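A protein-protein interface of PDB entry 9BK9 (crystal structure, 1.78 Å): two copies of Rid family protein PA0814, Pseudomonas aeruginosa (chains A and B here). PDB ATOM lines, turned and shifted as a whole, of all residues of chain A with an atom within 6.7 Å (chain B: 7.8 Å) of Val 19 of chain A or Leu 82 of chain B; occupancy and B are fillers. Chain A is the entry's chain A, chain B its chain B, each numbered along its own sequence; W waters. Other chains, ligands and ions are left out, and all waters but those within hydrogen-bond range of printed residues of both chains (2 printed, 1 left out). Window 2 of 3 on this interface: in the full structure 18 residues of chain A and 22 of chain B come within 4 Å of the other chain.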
ATOM      1  N   GLN A  16      36.481  26.985  23.702  1.00  0.00           N
ATOM      2  CA  GLN A  16      36.947  28.140  22.946  1.00  0.00           C
ATOM      3  C   GLN A  16      36.081  29.357  23.255  1.00  0.00           C
ATOM      4  O   GLN A  16      34.876  29.215  23.482  1.00  0.00           O
ATOM      5  CB  GLN A  16      36.893  27.843  21.448  1.00  0.00           C
ATOM      6  CG  GLN A  16      37.824  26.711  21.025  1.00  0.00           C
ATOM      7  CD  GLN A  16      39.298  27.080  21.099  1.00  0.00           C
ATOM      8  OE1 GLN A  16      39.682  28.212  20.811  1.00  0.00           O
ATOM      9  NE2 GLN A  16      40.132  26.112  21.454  1.00  0.00           N
ATOM     10  N   PRO A  17      36.650  30.561  23.288  1.00  0.00           N
ATOM     11  CA  PRO A  17      35.821  31.757  23.526  1.00  0.00           C
ATOM     12  C   PRO A  17      34.781  32.002  22.455  1.00  0.00           C
ATOM     13  O   PRO A  17      33.696  32.512  22.764  1.00  0.00           O
ATOM     14  CB  PRO A  17      36.852  32.897  23.578  1.00  0.00           C
ATOM     15  CG  PRO A  17      38.132  32.230  23.901  1.00  0.00           C
ATOM     16  CD  PRO A  17      38.087  30.875  23.259  1.00  0.00           C
ATOM     17  N   VAL A  18      35.112  31.725  21.194  1.00  0.00           N
ATOM     18  CA  VAL A  18      34.227  31.955  20.057  1.00  0.00           C
ATOM     19  C   VAL A  18      34.418  30.830  19.051  1.00  0.00           C
ATOM     20  O   VAL A  18      35.555  30.462  18.734  1.00  0.00           O
ATOM     21  CB  VAL A  18      34.504  33.308  19.356  1.00  0.00           C
ATOM     22  CG1 VAL A  18      33.566  33.484  18.198  1.00  0.00           C
ATOM     23  CG2 VAL A  18      34.411  34.488  20.328  1.00  0.00           C
ATOM     24  N   VAL A  19      33.316  30.324  18.502  1.00  0.00           N
ATOM     25  CA  VAL A  19      33.357  29.414  17.357  1.00  0.00           C
ATOM     26  C   VAL A  19      32.683  30.083  16.165  1.00  0.00           C
ATOM     27  O   VAL A  19      31.570  30.601  16.291  1.00  0.00           O
ATOM     28  CB  VAL A  19      32.672  28.070  17.669  1.00  0.00           C
ATOM     29  CG1 VAL A  19      32.473  27.253  16.370  1.00  0.00           C
ATOM     30  CG2 VAL A  19      33.502  27.293  18.665  1.00  0.00           C
ATOM     31  N   LEU A  20      33.352  30.073  15.006  1.00  0.00           N
ATOM     32  CA  LEU A  20      32.765  30.578  13.769  1.00  0.00           C
ATOM     33  C   LEU A  20      32.424  29.397  12.874  1.00  0.00           C
ATOM     34  O   LEU A  20      33.276  28.532  12.646  1.00  0.00           O
ATOM     35  CB  LEU A  20      33.719  31.524  13.026  1.00  0.00           C
ATOM     36  CG  LEU A  20      34.283  32.684  13.845  1.00  0.00           C
ATOM     37  CD1 LEU A  20      35.360  33.435  13.064  1.00  0.00           C
ATOM     38  CD2 LEU A  20      33.167  33.611  14.236  1.00  0.00           C
ATOM     39  N   HIS A  21      31.178  29.345  12.396  1.00  0.00           N
ATOM     40  CA  HIS A  21      30.756  28.274  11.497  1.00  0.00           C
ATOM     41  C   HIS A  21      29.582  28.734  10.644  1.00  0.00           C
ATOM     42  O   HIS A  21      28.582  29.228  11.169  1.00  0.00           O
ATOM     43  CB  HIS A  21      30.373  27.002  12.265  1.00  0.00           C
ATOM     44  CG  HIS A  21      29.900  25.890  11.377  1.00  0.00           C
ATOM     45  ND1 HIS A  21      30.765  25.101  10.651  1.00  0.00           N
ATOM     46  CD2 HIS A  21      28.653  25.449  11.085  1.00  0.00           C
ATOM     47  CE1 HIS A  21      30.072  24.217   9.954  1.00  0.00           C
ATOM     48  NE2 HIS A  21      28.788  24.411  10.194  1.00  0.00           N
ATOM     49  N   ILE A  24      27.827  32.044  11.269  1.00  0.00           N
ATOM     50  CA  ILE A  24      27.351  32.279  12.628  1.00  0.00           C
ATOM     51  C   ILE A  24      28.537  32.253  13.584  1.00  0.00           C
ATOM     52  O   ILE A  24      29.410  31.383  13.474  1.00  0.00           O
ATOM     53  CB  ILE A  24      26.317  31.213  13.042  1.00  0.00           C
ATOM     54  CG1 ILE A  24      25.166  31.145  12.033  1.00  0.00           C
ATOM     55  CG2 ILE A  24      25.814  31.476  14.459  1.00  0.00           C
ATOM     56  CD1 ILE A  24      24.337  32.413  11.938  1.00  0.00           C
ATOM     57  N   ALA A  25      28.553  33.186  14.543  1.00  0.00           N
ATOM     58  CA  ALA A  25      29.522  33.198  15.628  1.00  0.00           C
ATOM     59  C   ALA A  25      28.803  32.838  16.916  1.00  0.00           C
ATOM     60  O   ALA A  25      27.782  33.453  17.251  1.00  0.00           O
ATOM     61  CB  ALA A  25      30.198  34.566  15.778  1.00  0.00           C
ATOM     62  N   TYR A  26      29.318  31.819  17.607  1.00  0.00           N
ATOM     63  CA  TYR A  26      28.822  31.392  18.914  1.00  0.00           C
ATOM     64  C   TYR A  26      29.834  31.877  19.939  1.00  0.00           C
ATOM     65  O   TYR A  26      30.991  31.442  19.923  1.00  0.00           O
ATOM     66  CB  TYR A  26      28.664  29.872  18.956  1.00  0.00           C
ATOM     67  CG  TYR A  26      27.797  29.329  17.825  1.00  0.00           C
ATOM     68  CD1 TYR A  26      28.347  29.038  16.583  1.00  0.00           C
ATOM     69  CD2 TYR A  26      26.436  29.124  18.004  1.00  0.00           C
ATOM     70  CE1 TYR A  26      27.566  28.566  15.542  1.00  0.00           C
ATOM     71  CE2 TYR A  26      25.640  28.638  16.967  1.00  0.00           C
ATOM     72  CZ  TYR A  26      26.216  28.358  15.743  1.00  0.00           C
ATOM     73  OH  TYR A  26      25.451  27.882  14.702  1.00  0.00           O
ATOM     74  N   VAL A  27      29.422  32.814  20.794  1.00  0.00           N
ATOM     75  CA  VAL A  27      30.299  33.431  21.770  1.00  0.00           C
ATOM     76  C   VAL A  27      29.973  32.862  23.142  1.00  0.00           C
ATOM     77  O   VAL A  27      28.837  33.003  23.636  1.00  0.00           O
ATOM     78  CB  VAL A  27      30.161  34.963  21.760  1.00  0.00           C
ATOM     79  CG1 VAL A  27      31.065  35.586  22.802  1.00  0.00           C
ATOM     80  CG2 VAL A  27      30.464  35.522  20.385  1.00  0.00           C
ATOM     81  N   SER A  28      31.004  32.285  23.762  1.00  0.00           N
ATOM     82  CA  SER A  28      30.932  31.686  25.086  1.00  0.00           C
ATOM     83  C   SER A  28      30.497  32.698  26.134  1.00  0.00           C
ATOM     84  O   SER A  28      30.689  33.910  25.992  1.00  0.00           O
ATOM     85  CB  SER A  28      32.299  31.131  25.490  1.00  0.00           C
ATOM     86  OG  SER A  28      32.669  30.016  24.703  1.00  0.00           O
ATOM     87  N   ALA A  71      38.210  37.276  17.466  1.00  0.00           N
ATOM     88  CA  ALA A  71      38.012  36.116  16.608  1.00  0.00           C
ATOM     89  C   ALA A  71      37.888  36.508  15.144  1.00  0.00           C
ATOM     90  O   ALA A  71      38.314  35.746  14.269  1.00  0.00           O
ATOM     91  CB  ALA A  71      36.770  35.329  17.036  1.00  0.00           C
ATOM     92  N   GLY B  23      21.724  21.404   8.342  1.00  0.00           N
ATOM     93  CA  GLY B  23      23.113  21.252   8.720  1.00  0.00           C
ATOM     94  C   GLY B  23      23.424  21.478  10.183  1.00  0.00           C
ATOM     95  O   GLY B  23      24.607  21.533  10.546  1.00  0.00           O
ATOM     96  N   ILE B  24      22.408  21.626  11.032  1.00  0.00           N
ATOM     97  CA  ILE B  24      22.598  21.818  12.463  1.00  0.00           C
ATOM     98  C   ILE B  24      21.841  20.729  13.212  1.00  0.00           C
ATOM     99  O   ILE B  24      20.728  20.355  12.831  1.00  0.00           O
ATOM    100  CB  ILE B  24      22.123  23.209  12.928  1.00  0.00           C
ATOM    101  CG1 ILE B  24      22.785  24.311  12.101  1.00  0.00           C
ATOM    102  CG2 ILE B  24      22.432  23.390  14.406  1.00  0.00           C
ATOM    103  CD1 ILE B  24      24.278  24.378  12.261  1.00  0.00           C
ATOM    104  N   ALA B  25      22.448  20.225  14.276  1.00  0.00           N
ATOM    105  CA  ALA B  25      21.814  19.297  15.199  1.00  0.00           C
ATOM    106  C   ALA B  25      21.597  20.017  16.519  1.00  0.00           C
ATOM    107  O   ALA B  25      22.553  20.548  17.105  1.00  0.00           O
ATOM    108  CB  ALA B  25      22.677  18.051  15.405  1.00  0.00           C
ATOM    109  N   TYR B  26      20.345  20.038  16.974  1.00  0.00           N
ATOM    110  CA  TYR B  26      19.973  20.614  18.261  1.00  0.00           C
ATOM    111  C   TYR B  26      19.755  19.452  19.216  1.00  0.00           C
ATOM    112  O   TYR B  26      18.820  18.668  19.032  1.00  0.00           O
ATOM    113  CB  TYR B  26      18.715  21.477  18.120  1.00  0.00           C
ATOM    114  CG  TYR B  26      18.864  22.566  17.072  1.00  0.00           C
ATOM    115  CD1 TYR B  26      18.597  22.309  15.729  1.00  0.00           C
ATOM    116  CD2 TYR B  26      19.304  23.845  17.422  1.00  0.00           C
ATOM    117  CE1 TYR B  26      18.745  23.302  14.757  1.00  0.00           C
ATOM    118  CE2 TYR B  26      19.465  24.844  16.457  1.00  0.00           C
ATOM    119  CZ  TYR B  26      19.187  24.563  15.127  1.00  0.00           C
ATOM    120  OH  TYR B  26      19.347  25.546  14.157  1.00  0.00           O
ATOM    121  N   VAL B  78      29.123  14.043  12.166  1.00  0.00           N
ATOM    122  CA  VAL B  78      29.359  15.269  12.924  1.00  0.00           C
ATOM    123  C   VAL B  78      30.519  16.015  12.284  1.00  0.00           C
ATOM    124  O   VAL B  78      31.637  15.497  12.207  1.00  0.00           O
ATOM    125  CB  VAL B  78      29.646  14.986  14.403  1.00  0.00           C
ATOM    126  CG1 VAL B  78      30.094  16.292  15.088  1.00  0.00           C
ATOM    127  CG2 VAL B  78      28.406  14.450  15.096  1.00  0.00           C
ATOM    128  N   GLU B  79      30.243  17.212  11.771  1.00  0.00           N
ATOM    129  CA  GLU B  79      31.315  18.054  11.258  1.00  0.00           C
ATOM    130  C   GLU B  79      32.109  18.691  12.397  1.00  0.00           C
ATOM    131  O   GLU B  79      33.345  18.633  12.411  1.00  0.00           O
ATOM    132  CB  GLU B  79      30.719  19.089  10.307  1.00  0.00           C
ATOM    133  CG  GLU B  79      31.704  20.014   9.682  1.00  0.00           C
ATOM    134  CD  GLU B  79      31.069  20.873   8.604  1.00  0.00           C
ATOM    135  OE1 GLU B  79      29.900  20.608   8.237  1.00  0.00           O
ATOM    136  OE2 GLU B  79      31.735  21.817   8.131  1.00  0.00           O
ATOM    137  N   ARG B  80      31.419  19.275  13.381  1.00  0.00           N
ATOM    138  CA  ARG B  80      32.080  19.776  14.582  1.00  0.00           C
ATOM    139  C   ARG B  80      31.005  20.143  15.594  1.00  0.00           C
ATOM    140  O   ARG B  80      29.867  20.432  15.227  1.00  0.00           O
ATOM    141  CB  ARG B  80      32.966  21.001  14.297  1.00  0.00           C
ATOM    142  CG  ARG B  80      32.223  22.211  13.711  1.00  0.00           C
ATOM    143  CD  ARG B  80      33.048  23.507  13.888  1.00  0.00           C
ATOM    144  NE  ARG B  80      33.468  23.649  15.278  1.00  0.00           N
ATOM    145  CZ  ARG B  80      34.519  24.342  15.695  1.00  0.00           C
ATOM    146  NH1 ARG B  80      35.257  25.054  14.856  1.00  0.00           N
ATOM    147  NH2 ARG B  80      34.864  24.286  16.981  1.00  0.00           N
ATOM    148  N   LEU B  81      31.380  20.142  16.868  1.00  0.00           N
ATOM    149  CA  LEU B  81      30.495  20.752  17.847  1.00  0.00           C
ATOM    150  C   LEU B  81      30.540  22.266  17.684  1.00  0.00           C
ATOM    151  O   LEU B  81      31.491  22.824  17.140  1.00  0.00           O
ATOM    152  CB  LEU B  81      30.902  20.370  19.268  1.00  0.00           C
ATOM    153  CG  LEU B  81      30.925  18.882  19.623  1.00  0.00           C
ATOM    154  CD1 LEU B  81      31.136  18.714  21.142  1.00  0.00           C
ATOM    155  CD2 LEU B  81      29.640  18.214  19.142  1.00  0.00           C
ATOM    156  N   LEU B  82      29.482  22.935  18.131  1.00  0.00           N
ATOM    157  CA  LEU B  82      29.413  24.386  18.043  1.00  0.00           C
ATOM    158  C   LEU B  82      29.297  25.030  19.412  1.00  0.00           C
ATOM    159  O   LEU B  82      30.091  25.923  19.749  1.00  0.00           O
ATOM    160  CB  LEU B  82      28.235  24.808  17.167  1.00  0.00           C
ATOM    161  CG  LEU B  82      28.317  24.290  15.725  1.00  0.00           C
ATOM    162  CD1 LEU B  82      27.031  24.597  14.983  1.00  0.00           C
ATOM    163  CD2 LEU B  82      29.525  24.914  15.029  1.00  0.00           C
ATOM    164  N   LYS B  83      28.317  24.618  20.214  1.00  0.00           N
ATOM    165  CA  LYS B  83      28.122  25.309  21.477  1.00  0.00           C
ATOM    166  C   LYS B  83      27.558  24.314  22.470  1.00  0.00           C
ATOM    167  O   LYS B  83      26.675  23.523  22.131  1.00  0.00           O
ATOM    168  CB  LYS B  83      27.194  26.538  21.315  1.00  0.00           C
ATOM    169  CG  LYS B  83      26.868  27.269  22.608  1.00  0.00           C
ATOM    170  CD  LYS B  83      28.166  27.847  23.091  1.00  0.00           C
ATOM    171  CE  LYS B  83      28.165  28.907  24.226  1.00  0.00           C
ATOM    172  NZ  LYS B  83      27.354  30.136  23.956  1.00  0.00           N
ATOM    173  N   VAL B  84      28.070  24.348  23.690  1.00  0.00           N
ATOM    174  CA  VAL B  84      27.596  23.476  24.759  1.00  0.00           C
ATOM    175  C   VAL B  84      27.078  24.370  25.877  1.00  0.00           C
ATOM    176  O   VAL B  84      27.719  25.371  26.210  1.00  0.00           O
ATOM    177  CB  VAL B  84      28.714  22.554  25.278  1.00  0.00           C
ATOM    178  CG1 VAL B  84      28.261  21.805  26.522  1.00  0.00           C
ATOM    179  CG2 VAL B  84      29.178  21.581  24.186  1.00  0.00           C
ATOM    180  N   ARG B 115      37.179  17.828  16.176  1.00  0.00           N
ATOM    181  CA  ARG B 115      35.776  18.130  15.919  1.00  0.00           C
ATOM    182  C   ARG B 115      35.030  18.428  17.216  1.00  0.00           C
ATOM    183  O   ARG B 115      33.878  18.881  17.174  1.00  0.00           O
ATOM    184  CB  ARG B 115      35.105  16.954  15.203  1.00  0.00           C
ATOM    185  CG  ARG B 115      35.601  16.669  13.777  1.00  0.00           C
ATOM    186  CD  ARG B 115      34.823  15.493  13.167  1.00  0.00           C
ATOM    187  NE  ARG B 115      35.085  14.267  13.911  1.00  0.00           N
ATOM    188  CZ  ARG B 115      34.255  13.236  13.997  1.00  0.00           C
ATOM    189  NH1 ARG B 115      33.062  13.260  13.428  1.00  0.00           N
ATOM    190  NH2 ARG B 115      34.624  12.161  14.689  1.00  0.00           N
ATOM    191  N   GLY B 116      35.652  18.169  18.360  1.00  0.00           N
ATOM    192  CA  GLY B 116      35.044  18.398  19.650  1.00  0.00           C
ATOM    193  C   GLY B 116      35.131  19.802  20.208  1.00  0.00           C
ATOM    194  O   GLY B 116      34.565  20.039  21.277  1.00  0.00           O
ATOM    195  N   GLY B 117      35.821  20.729  19.551  1.00  0.00           N
ATOM    196  CA  GLY B 117      35.925  22.080  20.087  1.00  0.00           C
ATOM    197  C   GLY B 117      34.587  22.799  20.100  1.00  0.00           C
ATOM    198  O   GLY B 117      33.755  22.631  19.208  1.00  0.00           O
ATOM    199  N   HIS B 118      34.386  23.651  21.105  1.00  0.00           N
ATOM    200  CA  HIS B 118      33.073  24.270  21.231  1.00  0.00           C
ATOM    201  C   HIS B 118      33.156  25.548  22.047  1.00  0.00           C
ATOM    202  O   HIS B 118      34.008  25.691  22.928  1.00  0.00           O
ATOM    203  CB  HIS B 118      32.087  23.316  21.898  1.00  0.00           C
ATOM    204  CG  HIS B 118      32.602  22.753  23.184  1.00  0.00           C
ATOM    205  ND1 HIS B 118      33.425  21.647  23.223  1.00  0.00           N
ATOM    206  CD2 HIS B 118      32.425  23.138  24.471  1.00  0.00           C
ATOM    207  CE1 HIS B 118      33.731  21.374  24.481  1.00  0.00           C
ATOM    208  NE2 HIS B 118      33.144  22.268  25.258  1.00  0.00           N
ATOM    209  N   ALA B 119      32.239  26.464  21.755  1.00  0.00           N
ATOM    210  CA  ALA B 119      31.951  27.518  22.711  1.00  0.00           C
ATOM    211  C   ALA B 119      31.120  26.936  23.853  1.00  0.00           C
ATOM    212  O   ALA B 119      30.545  25.850  23.736  1.00  0.00           O
ATOM    213  CB  ALA B 119      31.228  28.683  22.034  1.00  0.00           C
ATOM    214  N   ARG B 120      31.053  27.660  24.969  1.00  0.00           N
ATOM    215  CA  ARG B 120      30.452  27.066  26.159  1.00  0.00           C
ATOM    216  C   ARG B 120      29.853  28.128  27.073  1.00  0.00           C
ATOM    217  O   ARG B 120      30.330  29.260  27.135  1.00  0.00           O
ATOM    218  CB  ARG B 120      31.488  26.266  26.956  1.00  0.00           C
ATOM    219  CG  ARG B 120      30.898  25.179  27.849  1.00  0.00           C
ATOM    220  CD  ARG B 120      32.012  24.420  28.561  1.00  0.00           C
ATOM    221  NE  ARG B 120      32.556  25.187  29.673  1.00  0.00           N
ATOM    222  CZ  ARG B 120      33.582  24.788  30.411  1.00  0.00           C
ATOM    223  NH1 ARG B 120      34.223  23.663  30.145  1.00  0.00           N
ATOM    224  NH2 ARG B 120      33.965  25.528  31.449  1.00  0.00           N
ATOM    225  N   LEU B 138      23.442  20.721  23.680  1.00  0.00           N
ATOM    226  CA  LEU B 138      24.462  21.208  22.759  1.00  0.00           C
ATOM    227  C   LEU B 138      23.895  21.450  21.367  1.00  0.00           C
ATOM    228  O   LEU B 138      22.809  20.992  21.023  1.00  0.00           O
ATOM    229  CB  LEU B 138      25.661  20.253  22.703  1.00  0.00           C
ATOM    230  CG  LEU B 138      25.609  18.877  22.035  1.00  0.00           C
ATOM    231  CD1 LEU B 138      25.732  18.983  20.511  1.00  0.00           C
ATOM    232  CD2 LEU B 138      26.706  17.978  22.596  1.00  0.00           C
ATOM    233  N   ILE B 139      24.665  22.196  20.580  1.00  0.00           N
ATOM    234  CA  ILE B 139      24.387  22.466  19.175  1.00  0.00           C
ATOM    235  C   ILE B 139      25.622  22.014  18.411  1.00  0.00           C
ATOM    236  O   ILE B 139      26.751  22.366  18.792  1.00  0.00           O
ATOM    237  CB  ILE B 139      24.121  23.967  18.916  1.00  0.00           C
ATOM    238  CG1 ILE B 139      22.870  24.457  19.652  1.00  0.00           C
ATOM    239  CG2 ILE B 139      23.940  24.241  17.421  1.00  0.00           C
ATOM    240  CD1 ILE B 139      22.809  25.999  19.778  1.00  0.00           C
ATOM    241  N   ALA B 140      25.411  21.261  17.325  1.00  0.00           N
ATOM    242  CA  ALA B 140      26.517  20.726  16.533  1.00  0.00           C
ATOM    243  C   ALA B 140      26.257  20.960  15.054  1.00  0.00           C
ATOM    244  O   ALA B 140      25.113  21.062  14.620  1.00  0.00           O
ATOM    245  CB  ALA B 140      26.723  19.226  16.785  1.00  0.00           C
ATOM    246  N   ALA B 141      27.332  21.012  14.273  1.00  0.00           N
ATOM    247  CA  ALA B 141      27.214  21.067  12.820  1.00  0.00           C
ATOM    248  C   ALA B 141      27.291  19.653  12.258  1.00  0.00           C
ATOM    249  O   ALA B 141      28.089  18.837  12.717  1.00  0.00           O
ATOM    250  CB  ALA B 141      28.309  21.947  12.205  1.00  0.00           C
ATOM    251  N   VAL B 142      26.426  19.352  11.289  1.00  0.00           N
ATOM    252  CA  VAL B 142      26.316  17.995  10.768  1.00  0.00           C
ATOM    253  C   VAL B 142      26.336  18.001   9.245  1.00  0.00           C
ATOM    254  O   VAL B 142      26.017  18.995   8.587  1.00  0.00           O
ATOM    255  CB  VAL B 142      25.065  17.253  11.297  1.00  0.00           C
ATOM    256  CG1 VAL B 142      25.199  17.010  12.808  1.00  0.00           C
ATOM    257  CG2 VAL B 142      23.799  18.027  10.987  1.00  0.00           C
HETATM  258  O   HOH W   1      26.318  22.830   8.949  1.00  0.00           O
HETATM  259  O   HOH W   2      34.543  26.215  12.550  1.00  0.00           O
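N of Gln 16 of chain A is in hydrogen-bond range of O of His 118 of chain B.
NZ of Lys 83 of chain B sits at hydrogen-bond distance from O of Val 27 of chain A (3.2 Å).
The backbone NH (N) of Arg 120 of chain B sits at hydrogen-bond distance from the side-chain hydroxyl (OG) of Ser 28 of chain A (2.9 Å).
O of Gln 16 of chain A lies within hydrogen-bond range of OG of Ser 28 of chain A (2.6 Å).
O of Pro 17 of chain A lies within hydrogen-bond range of N of Ser 28 of chain A.
O of Ala 141 of chain B sits at hydrogen-bond distance from N of Glu 79 of chain B (2.9 Å).
The backbone NH of Ala 141 of chain B is in hydrogen-bond range of the backbone carbonyl oxygen of Arg 80 of chain B (2.8 Å).
The backbone NH (N) of Ala 119 of chain B is in hydrogen-bond range of the backbone carbonyl oxygen (O) of Leu 82 of chain B (3.0 Å).
N of Leu 82 of chain B is in hydrogen-bond range of O of Ile 139 of chain B (2.9 Å).
Among the printed residues, merely in contact across the chains: Gln 16 of chain A with Ala 119 of chain B (3.5 Å), Val 19 of chain A with Arg 80 of chain B (3.6 Å), Val 19 of chain A with Leu 82 of chain B (3.8 Å), Val 19 of chain A with His 118 of chain B (3.8 Å), Val 19 of chain A with Ala 119 of chain B (3.4 Å), His 21 of chain A with Glu 79 of chain B (3.4 Å), His 21 of chain A with Leu 82 of chain B (3.6 Å), His 21 of chain A with Ala 141 of chain B (3.2 Å), Tyr 26 of chain A with Leu 82 of chain B (3.7 Å), Tyr 26 of chain A with Ala 119 of chain B (3.5 Å) and Ser 28 of chain A with Ala 119 of chain B (3.3 Å).
Val 19 of chain A touches just these residues of chain B: Arg 80, Leu 82, His 118 and Ala 119.
Of chain A, only Val 19 (3.8 Å), His 21 (3.6 Å) and Tyr 26 (3.7 Å) come within 4 Å of Leu 82 of chain B.
Of the printed residues of chain B, Gln 16 of chain A touches His 118 and Ala 119.
Of the printed residues of chain B, Tyr 26 of chain A touches Leu 82 (3.7 Å) and Ala 119 (3.5 Å).
The nearest residue of chain A that does not touch Leu 82 of chain B is Leu 20 of chain A (5.7 Å).
Of the 22 printed residues of chain B, 8 touch a printed residue of chain A.
Positions printed for both chains: 24, 25 and 26.
Water W2 lies within hydrogen-bond range of the backbone carbonyl oxygen (O) of Leu 20 of chain A (2.6 Å) and the guanidinium group (NH1) of Arg 80 of chain B (2.7 Å).
Water W1 bridges O of Gly 23 of chain B (2.7 Å) and NE2 of His 21 of chain A (3.2 Å).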
